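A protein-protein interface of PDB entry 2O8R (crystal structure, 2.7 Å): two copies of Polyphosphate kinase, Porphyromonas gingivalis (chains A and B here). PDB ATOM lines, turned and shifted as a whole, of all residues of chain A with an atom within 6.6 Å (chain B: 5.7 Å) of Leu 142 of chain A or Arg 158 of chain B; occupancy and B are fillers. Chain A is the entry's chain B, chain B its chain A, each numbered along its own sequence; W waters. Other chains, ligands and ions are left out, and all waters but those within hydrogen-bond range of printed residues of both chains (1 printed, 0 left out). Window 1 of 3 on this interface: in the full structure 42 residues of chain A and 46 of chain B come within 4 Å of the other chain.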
ATOM      1  N   GLU A 138      11.535  -3.294 -28.047  1.00  0.00           N
ATOM      2  CA  GLU A 138      10.226  -3.746 -28.530  1.00  0.00           C
ATOM      3  C   GLU A 138       9.378  -4.425 -27.472  1.00  0.00           C
ATOM      4  O   GLU A 138       8.183  -4.174 -27.396  1.00  0.00           O
ATOM      5  CB  GLU A 138      10.386  -4.726 -29.697  1.00  0.00           C
ATOM      6  CG  GLU A 138      11.512  -4.413 -30.645  1.00  0.00           C
ATOM      7  CD  GLU A 138      11.078  -3.579 -31.824  1.00  0.00           C
ATOM      8  OE1 GLU A 138      10.136  -2.765 -31.684  1.00  0.00           O
ATOM      9  OE2 GLU A 138      11.694  -3.747 -32.899  1.00  0.00           O
ATOM     10  N   ILE A 139       9.988  -5.315 -26.691  1.00  0.00           N
ATOM     11  CA  ILE A 139       9.261  -6.066 -25.674  1.00  0.00           C
ATOM     12  C   ILE A 139       9.034  -5.264 -24.397  1.00  0.00           C
ATOM     13  O   ILE A 139       7.911  -5.167 -23.922  1.00  0.00           O
ATOM     14  CB  ILE A 139       9.962  -7.374 -25.298  1.00  0.00           C
ATOM     15  CG1 ILE A 139      10.202  -8.214 -26.545  1.00  0.00           C
ATOM     16  CG2 ILE A 139       9.115  -8.148 -24.258  1.00  0.00           C
ATOM     17  CD1 ILE A 139      10.760  -9.595 -26.268  1.00  0.00           C
ATOM     18  N   PHE A 140      10.105  -4.707 -23.841  1.00  0.00           N
ATOM     19  CA  PHE A 140      10.027  -4.028 -22.553  1.00  0.00           C
ATOM     20  C   PHE A 140       8.911  -2.979 -22.487  1.00  0.00           C
ATOM     21  O   PHE A 140       8.030  -3.088 -21.637  1.00  0.00           O
ATOM     22  CB  PHE A 140      11.387  -3.464 -22.119  1.00  0.00           C
ATOM     23  CG  PHE A 140      11.383  -2.865 -20.739  1.00  0.00           C
ATOM     24  CD1 PHE A 140      11.450  -3.679 -19.615  1.00  0.00           C
ATOM     25  CD2 PHE A 140      11.312  -1.486 -20.563  1.00  0.00           C
ATOM     26  CE1 PHE A 140      11.448  -3.132 -18.335  1.00  0.00           C
ATOM     27  CE2 PHE A 140      11.313  -0.932 -19.282  1.00  0.00           C
ATOM     28  CZ  PHE A 140      11.378  -1.756 -18.167  1.00  0.00           C
ATOM     29  N   PRO A 141       8.908  -1.987 -23.399  1.00  0.00           N
ATOM     30  CA  PRO A 141       7.834  -0.981 -23.333  1.00  0.00           C
ATOM     31  C   PRO A 141       6.404  -1.541 -23.395  1.00  0.00           C
ATOM     32  O   PRO A 141       5.462  -0.820 -23.114  1.00  0.00           O
ATOM     33  CB  PRO A 141       8.101  -0.097 -24.556  1.00  0.00           C
ATOM     34  CG  PRO A 141       9.545  -0.291 -24.857  1.00  0.00           C
ATOM     35  CD  PRO A 141       9.842  -1.712 -24.507  1.00  0.00           C
ATOM     36  N   LEU A 142       6.250  -2.812 -23.739  1.00  0.00           N
ATOM     37  CA  LEU A 142       4.929  -3.439 -23.778  1.00  0.00           C
ATOM     38  C   LEU A 142       4.635  -4.277 -22.545  1.00  0.00           C
ATOM     39  O   LEU A 142       3.636  -5.013 -22.520  1.00  0.00           O
ATOM     40  CB  LEU A 142       4.803  -4.331 -25.002  1.00  0.00           C
ATOM     41  CG  LEU A 142       4.907  -3.641 -26.353  1.00  0.00           C
ATOM     42  CD1 LEU A 142       4.341  -4.593 -27.352  1.00  0.00           C
ATOM     43  CD2 LEU A 142       4.132  -2.312 -26.345  1.00  0.00           C
ATOM     44  N   LEU A 143       5.501  -4.160 -21.533  1.00  0.00           N
ATOM     45  CA  LEU A 143       5.414  -4.977 -20.321  1.00  0.00           C
ATOM     46  C   LEU A 143       4.774  -4.235 -19.163  1.00  0.00           C
ATOM     47  O   LEU A 143       4.985  -3.026 -18.996  1.00  0.00           O
ATOM     48  CB  LEU A 143       6.803  -5.461 -19.904  1.00  0.00           C
ATOM     49  CG  LEU A 143       7.488  -6.486 -20.821  1.00  0.00           C
ATOM     50  CD1 LEU A 143       8.707  -7.044 -20.142  1.00  0.00           C
ATOM     51  CD2 LEU A 143       6.543  -7.632 -21.203  1.00  0.00           C
ATOM     52  N   TYR A 144       3.990  -4.958 -18.362  1.00  0.00           N
ATOM     53  CA  TYR A 144       3.477  -4.395 -17.109  1.00  0.00           C
ATOM     54  C   TYR A 144       3.880  -5.257 -15.915  1.00  0.00           C
ATOM     55  O   TYR A 144       3.088  -6.066 -15.440  1.00  0.00           O
ATOM     56  CB  TYR A 144       1.958  -4.272 -17.126  1.00  0.00           C
ATOM     57  CG  TYR A 144       1.339  -3.415 -18.208  1.00  0.00           C
ATOM     58  CD1 TYR A 144       1.223  -2.039 -18.050  1.00  0.00           C
ATOM     59  CD2 TYR A 144       0.795  -3.994 -19.356  1.00  0.00           C
ATOM     60  CE1 TYR A 144       0.625  -1.252 -19.025  1.00  0.00           C
ATOM     61  CE2 TYR A 144       0.182  -3.217 -20.332  1.00  0.00           C
ATOM     62  CZ  TYR A 144       0.098  -1.847 -20.163  1.00  0.00           C
ATOM     63  OH  TYR A 144      -0.507  -1.067 -21.126  1.00  0.00           O
ATOM     64  N   ASN A 183       3.046  -9.999 -18.236  1.00  0.00           N
ATOM     65  CA  ASN A 183       2.354 -10.230 -19.510  1.00  0.00           C
ATOM     66  C   ASN A 183       3.301 -10.729 -20.583  1.00  0.00           C
ATOM     67  O   ASN A 183       4.477 -10.402 -20.572  1.00  0.00           O
ATOM     68  CB  ASN A 183       1.609  -8.982 -20.010  1.00  0.00           C
ATOM     69  CG  ASN A 183       2.467  -7.724 -20.006  1.00  0.00           C
ATOM     70  OD1 ASN A 183       3.076  -7.371 -19.001  1.00  0.00           O
ATOM     71  ND2 ASN A 183       2.469  -7.011 -21.123  1.00  0.00           N
ATOM     72  N   VAL A 184       2.778 -11.538 -21.501  1.00  0.00           N
ATOM     73  CA  VAL A 184       3.502 -11.900 -22.713  1.00  0.00           C
ATOM     74  C   VAL A 184       2.761 -11.227 -23.860  1.00  0.00           C
ATOM     75  O   VAL A 184       1.752 -11.757 -24.341  1.00  0.00           O
ATOM     76  CB  VAL A 184       3.559 -13.421 -22.901  1.00  0.00           C
ATOM     77  CG1 VAL A 184       4.306 -13.784 -24.179  1.00  0.00           C
ATOM     78  CG2 VAL A 184       4.217 -14.067 -21.690  1.00  0.00           C
ATOM     79  N   PRO A 185       3.264 -10.060 -24.314  1.00  0.00           N
ATOM     80  CA  PRO A 185       2.467  -9.121 -25.106  1.00  0.00           C
ATOM     81  C   PRO A 185       2.344  -9.557 -26.560  1.00  0.00           C
ATOM     82  O   PRO A 185       2.944  -8.966 -27.455  1.00  0.00           O
ATOM     83  CB  PRO A 185       3.243  -7.807 -24.981  1.00  0.00           C
ATOM     84  CG  PRO A 185       4.637  -8.199 -24.712  1.00  0.00           C
ATOM     85  CD  PRO A 185       4.652  -9.598 -24.150  1.00  0.00           C
ATOM     86  N   ASP A 187      -0.268  -9.373 -28.300  1.00  0.00           N
ATOM     87  CA  ASP A 187      -1.231  -8.484 -28.924  1.00  0.00           C
ATOM     88  C   ASP A 187      -0.514  -7.354 -29.668  1.00  0.00           C
ATOM     89  O   ASP A 187      -1.130  -6.623 -30.454  1.00  0.00           O
ATOM     90  CB  ASP A 187      -2.144  -7.883 -27.844  1.00  0.00           C
ATOM     91  CG  ASP A 187      -1.361  -7.187 -26.725  1.00  0.00           C
ATOM     92  OD1 ASP A 187      -0.318  -7.717 -26.297  1.00  0.00           O
ATOM     93  OD2 ASP A 187      -1.798  -6.115 -26.258  1.00  0.00           O
ATOM     94  N   GLY A 188       0.781  -7.201 -29.391  1.00  0.00           N
ATOM     95  CA  GLY A 188       1.594  -6.177 -30.034  1.00  0.00           C
ATOM     96  C   GLY A 188       2.798  -6.757 -30.752  1.00  0.00           C
ATOM     97  O   GLY A 188       3.488  -6.048 -31.486  1.00  0.00           O
ATOM     98  N   LEU A 189       3.051  -8.045 -30.539  1.00  0.00           N
ATOM     99  CA  LEU A 189       4.237  -8.706 -31.072  1.00  0.00           C
ATOM    100  C   LEU A 189       3.910 -10.165 -31.431  1.00  0.00           C
ATOM    101  O   LEU A 189       3.030 -10.764 -30.834  1.00  0.00           O
ATOM    102  CB  LEU A 189       5.363  -8.654 -30.030  1.00  0.00           C
ATOM    103  CG  LEU A 189       6.141  -7.347 -29.866  1.00  0.00           C
ATOM    104  CD1 LEU A 189       7.113  -7.403 -28.683  1.00  0.00           C
ATOM    105  CD2 LEU A 189       6.892  -7.052 -31.151  1.00  0.00           C
ATOM    106  N   PHE B 156       8.201   0.664 -17.188  1.00  0.00           N
ATOM    107  CA  PHE B 156       8.216   1.627 -18.280  1.00  0.00           C
ATOM    108  C   PHE B 156       6.918   2.424 -18.264  1.00  0.00           C
ATOM    109  O   PHE B 156       5.878   1.920 -17.849  1.00  0.00           O
ATOM    110  CB  PHE B 156       8.335   0.883 -19.608  1.00  0.00           C
ATOM    111  CG  PHE B 156       8.697   1.754 -20.766  1.00  0.00           C
ATOM    112  CD1 PHE B 156      10.022   2.114 -20.990  1.00  0.00           C
ATOM    113  CD2 PHE B 156       7.721   2.213 -21.642  1.00  0.00           C
ATOM    114  CE1 PHE B 156      10.367   2.924 -22.060  1.00  0.00           C
ATOM    115  CE2 PHE B 156       8.060   3.017 -22.725  1.00  0.00           C
ATOM    116  CZ  PHE B 156       9.387   3.371 -22.935  1.00  0.00           C
ATOM    117  N   ILE B 157       6.982   3.672 -18.706  1.00  0.00           N
ATOM    118  CA  ILE B 157       5.789   4.489 -18.905  1.00  0.00           C
ATOM    119  C   ILE B 157       5.786   4.959 -20.358  1.00  0.00           C
ATOM    120  O   ILE B 157       6.593   5.805 -20.736  1.00  0.00           O
ATOM    121  CB  ILE B 157       5.763   5.700 -17.941  1.00  0.00           C
ATOM    122  CG1 ILE B 157       5.698   5.224 -16.494  1.00  0.00           C
ATOM    123  CG2 ILE B 157       4.583   6.621 -18.224  1.00  0.00           C
ATOM    124  CD1 ILE B 157       5.716   6.348 -15.473  1.00  0.00           C
ATOM    125  N   ARG B 158       4.892   4.392 -21.165  1.00  0.00           N
ATOM    126  CA  ARG B 158       4.826   4.691 -22.603  1.00  0.00           C
ATOM    127  C   ARG B 158       4.357   6.107 -22.903  1.00  0.00           C
ATOM    128  O   ARG B 158       3.605   6.721 -22.132  1.00  0.00           O
ATOM    129  CB  ARG B 158       3.909   3.707 -23.321  1.00  0.00           C
ATOM    130  CG  ARG B 158       4.266   2.261 -23.081  1.00  0.00           C
ATOM    131  CD  ARG B 158       3.318   1.361 -23.802  1.00  0.00           C
ATOM    132  NE  ARG B 158       3.374   1.515 -25.254  1.00  0.00           N
ATOM    133  CZ  ARG B 158       2.518   0.929 -26.090  1.00  0.00           C
ATOM    134  NH1 ARG B 158       1.542   0.165 -25.609  1.00  0.00           N
ATOM    135  NH2 ARG B 158       2.625   1.108 -27.401  1.00  0.00           N
ATOM    136  N   SER B 159       4.808   6.616 -24.041  1.00  0.00           N
ATOM    137  CA  SER B 159       4.478   7.965 -24.433  1.00  0.00           C
ATOM    138  C   SER B 159       3.109   7.989 -25.094  1.00  0.00           C
ATOM    139  O   SER B 159       2.617   6.959 -25.579  1.00  0.00           O
ATOM    140  CB  SER B 159       5.561   8.558 -25.341  1.00  0.00           C
ATOM    141  OG  SER B 159       5.717   7.788 -26.514  1.00  0.00           O
ATOM    142  N   GLY B 160       2.484   9.164 -25.067  1.00  0.00           N
ATOM    143  CA  GLY B 160       1.187   9.381 -25.702  1.00  0.00           C
ATOM    144  C   GLY B 160       0.027   8.759 -24.959  1.00  0.00           C
ATOM    145  O   GLY B 160      -1.121   8.910 -25.361  1.00  0.00           O
ATOM    146  N   ARG B 161       0.332   8.047 -23.878  1.00  0.00           N
ATOM    147  CA  ARG B 161      -0.690   7.429 -23.044  1.00  0.00           C
ATOM    148  C   ARG B 161      -0.906   8.235 -21.759  1.00  0.00           C
ATOM    149  O   ARG B 161      -0.126   9.135 -21.430  1.00  0.00           O
ATOM    150  CB  ARG B 161      -0.314   5.977 -22.720  1.00  0.00           C
ATOM    151  CG  ARG B 161      -0.134   5.076 -23.940  1.00  0.00           C
ATOM    152  CD  ARG B 161      -1.465   4.706 -24.594  1.00  0.00           C
ATOM    153  NE  ARG B 161      -2.001   3.419 -24.136  1.00  0.00           N
ATOM    154  CZ  ARG B 161      -2.903   3.283 -23.167  1.00  0.00           C
ATOM    155  NH1 ARG B 161      -3.368   4.352 -22.534  1.00  0.00           N
ATOM    156  NH2 ARG B 161      -3.341   2.079 -22.825  1.00  0.00           N
ATOM    157  N   TYR B 163      -1.346   7.750 -17.671  1.00  0.00           N
ATOM    158  CA  TYR B 163      -1.238   6.846 -16.529  1.00  0.00           C
ATOM    159  C   TYR B 163      -1.677   7.566 -15.270  1.00  0.00           C
ATOM    160  O   TYR B 163      -1.665   8.808 -15.191  1.00  0.00           O
ATOM    161  CB  TYR B 163       0.192   6.369 -16.320  1.00  0.00           C
ATOM    162  CG  TYR B 163       0.764   5.470 -17.380  1.00  0.00           C
ATOM    163  CD1 TYR B 163       1.070   4.145 -17.096  1.00  0.00           C
ATOM    164  CD2 TYR B 163       1.035   5.947 -18.658  1.00  0.00           C
ATOM    165  CE1 TYR B 163       1.622   3.319 -18.061  1.00  0.00           C
ATOM    166  CE2 TYR B 163       1.585   5.124 -19.635  1.00  0.00           C
ATOM    167  CZ  TYR B 163       1.872   3.812 -19.332  1.00  0.00           C
ATOM    168  OH  TYR B 163       2.423   2.995 -20.297  1.00  0.00           O
ATOM    169  N   ASP B 187      -6.455   2.054 -25.245  1.00  0.00           N
ATOM    170  CA  ASP B 187      -6.190   1.163 -26.358  1.00  0.00           C
ATOM    171  C   ASP B 187      -7.322   0.153 -26.538  1.00  0.00           C
ATOM    172  O   ASP B 187      -7.345  -0.594 -27.509  1.00  0.00           O
ATOM    173  CB  ASP B 187      -4.870   0.427 -26.118  1.00  0.00           C
ATOM    174  CG  ASP B 187      -4.809  -0.262 -24.748  1.00  0.00           C
ATOM    175  OD1 ASP B 187      -5.831  -0.302 -24.029  1.00  0.00           O
ATOM    176  OD2 ASP B 187      -3.722  -0.766 -24.387  1.00  0.00           O
ATOM    177  N   VAL B 234       4.080  11.220 -20.386  1.00  0.00           N
ATOM    178  CA  VAL B 234       5.442  11.504 -20.809  1.00  0.00           C
ATOM    179  C   VAL B 234       5.484  11.536 -22.324  1.00  0.00           C
ATOM    180  O   VAL B 234       4.888  10.687 -22.968  1.00  0.00           O
ATOM    181  CB  VAL B 234       6.460  10.476 -20.212  1.00  0.00           C
ATOM    182  CG1 VAL B 234       5.984   9.055 -20.392  1.00  0.00           C
ATOM    183  CG2 VAL B 234       7.847  10.650 -20.801  1.00  0.00           C
ATOM    184  N   ARG B 236       8.310  11.233 -25.294  1.00  0.00           N
ATOM    185  CA  ARG B 236       9.730  10.936 -25.526  1.00  0.00           C
ATOM    186  C   ARG B 236      10.087  10.848 -27.010  1.00  0.00           C
ATOM    187  O   ARG B 236       9.192  10.763 -27.858  1.00  0.00           O
ATOM    188  CB  ARG B 236      10.179   9.685 -24.764  1.00  0.00           C
ATOM    189  CG  ARG B 236       9.299   8.464 -24.920  1.00  0.00           C
ATOM    190  CD  ARG B 236       9.855   7.328 -24.090  1.00  0.00           C
ATOM    191  NE  ARG B 236      10.051   7.735 -22.706  1.00  0.00           N
ATOM    192  CZ  ARG B 236       9.534   7.094 -21.665  1.00  0.00           C
ATOM    193  NH1 ARG B 236       8.810   6.010 -21.859  1.00  0.00           N
ATOM    194  NH2 ARG B 236       9.751   7.525 -20.431  1.00  0.00           N
ATOM    195  N   ASP B 239       9.824   5.285 -28.071  1.00  0.00           N
ATOM    196  CA  ASP B 239       9.527   4.358 -26.973  1.00  0.00           C
ATOM    197  C   ASP B 239      10.515   3.203 -26.916  1.00  0.00           C
ATOM    198  O   ASP B 239      10.322   2.183 -27.586  1.00  0.00           O
ATOM    199  CB  ASP B 239       8.110   3.790 -27.098  1.00  0.00           C
ATOM    200  CG  ASP B 239       7.070   4.635 -26.383  1.00  0.00           C
ATOM    201  OD1 ASP B 239       7.422   5.741 -25.892  1.00  0.00           O
ATOM    202  OD2 ASP B 239       5.901   4.179 -26.317  1.00  0.00           O
HETATM  203  O   HOH W   1      -2.392  -2.493 -22.290  1.00  0.00           O
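The backbone NH (N) of Arg 158 of chain B is in hydrogen-bond range of the side-chain hydroxyl (OH) of Tyr 163 of chain B.
The guanidinium group (NE) of Arg 158 of chain B is in salt-bridge range of the side-chain carboxylate (OD2) of Asp 239 of chain B (3.8 Å).
The side-chain hydroxyl of Ser 159 of chain B is in hydrogen-bond range of the side-chain carboxylate of Asp 239 of chain B, 2.7 Å away.
The backbone carbonyl oxygen (O) of Leu 142 of chain A is in hydrogen-bond range of the side-chain amide nitrogen (ND2) of Asn 183 of chain A (2.7 Å).
Phe 140 of chain A touches Phe 156 of chain B (CE2 to CB, 3.5 Å).
Phe 156 of chain B touches Pro 141 of chain A (CE2 to CB, 3.6 Å).
Arg 158 of chain B touches Pro 141 of chain A (CD to O, 3.1 Å).
Asp 239 of chain B touches Pro 141 of chain A.
Arg 158 of chain B touches Leu 142 of chain A.
Of the printed residues of chain B, Phe 140 of chain A touches Phe 156.
Of chain B, only Arg 158 (3.6 Å) comes within 4 Å of Leu 142 of chain A.
Printed residues of chain A within 4 Å of Phe 156 of chain B: Phe 140 (3.5 Å) and Pro 141 (3.6 Å).
Printed residues of chain A within 4 Å of Arg 158 of chain B: Pro 141 and Leu 142.
Tyr 163 of chain B touches none of the printed residues of chain A.
Of the printed residues of chain A, Asp 239 of chain B touches Pro 141 (3.8 Å).
The nearest residue of chain A that does not touch Arg 158 of chain B is Tyr 144 of chain A (5.1 Å).
Hydrophobic or aromatic side chains of chain B that line the printed part of chain A: Phe 156.
Printed residues of chain A that touch a printed residue of chain B: Phe 140, Pro 141 and Leu 142.
Hydrophobic or aromatic side chains of chain A within 4 Å of the printed part of chain B: Phe 140, Pro 141 and Leu 142.
Along chain A the printed residues that touch a printed residue of chain B span positions 140 to 142.
Among the printed residues, no Asp or Glu carboxylate lies within 4 Å of a Lys or Arg side-chain nitrogen of the other chain.
1 position is printed for both chains.
Of the 5 pairs that touch across the chains among the printed residues, none has its exchanged pair printed and touching as well.
Water W1 lies within hydrogen-bond range of OH of Tyr 144 of chain A (2.6 Å) and OD2 of Asp 187 of chain B (3.0 Å).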
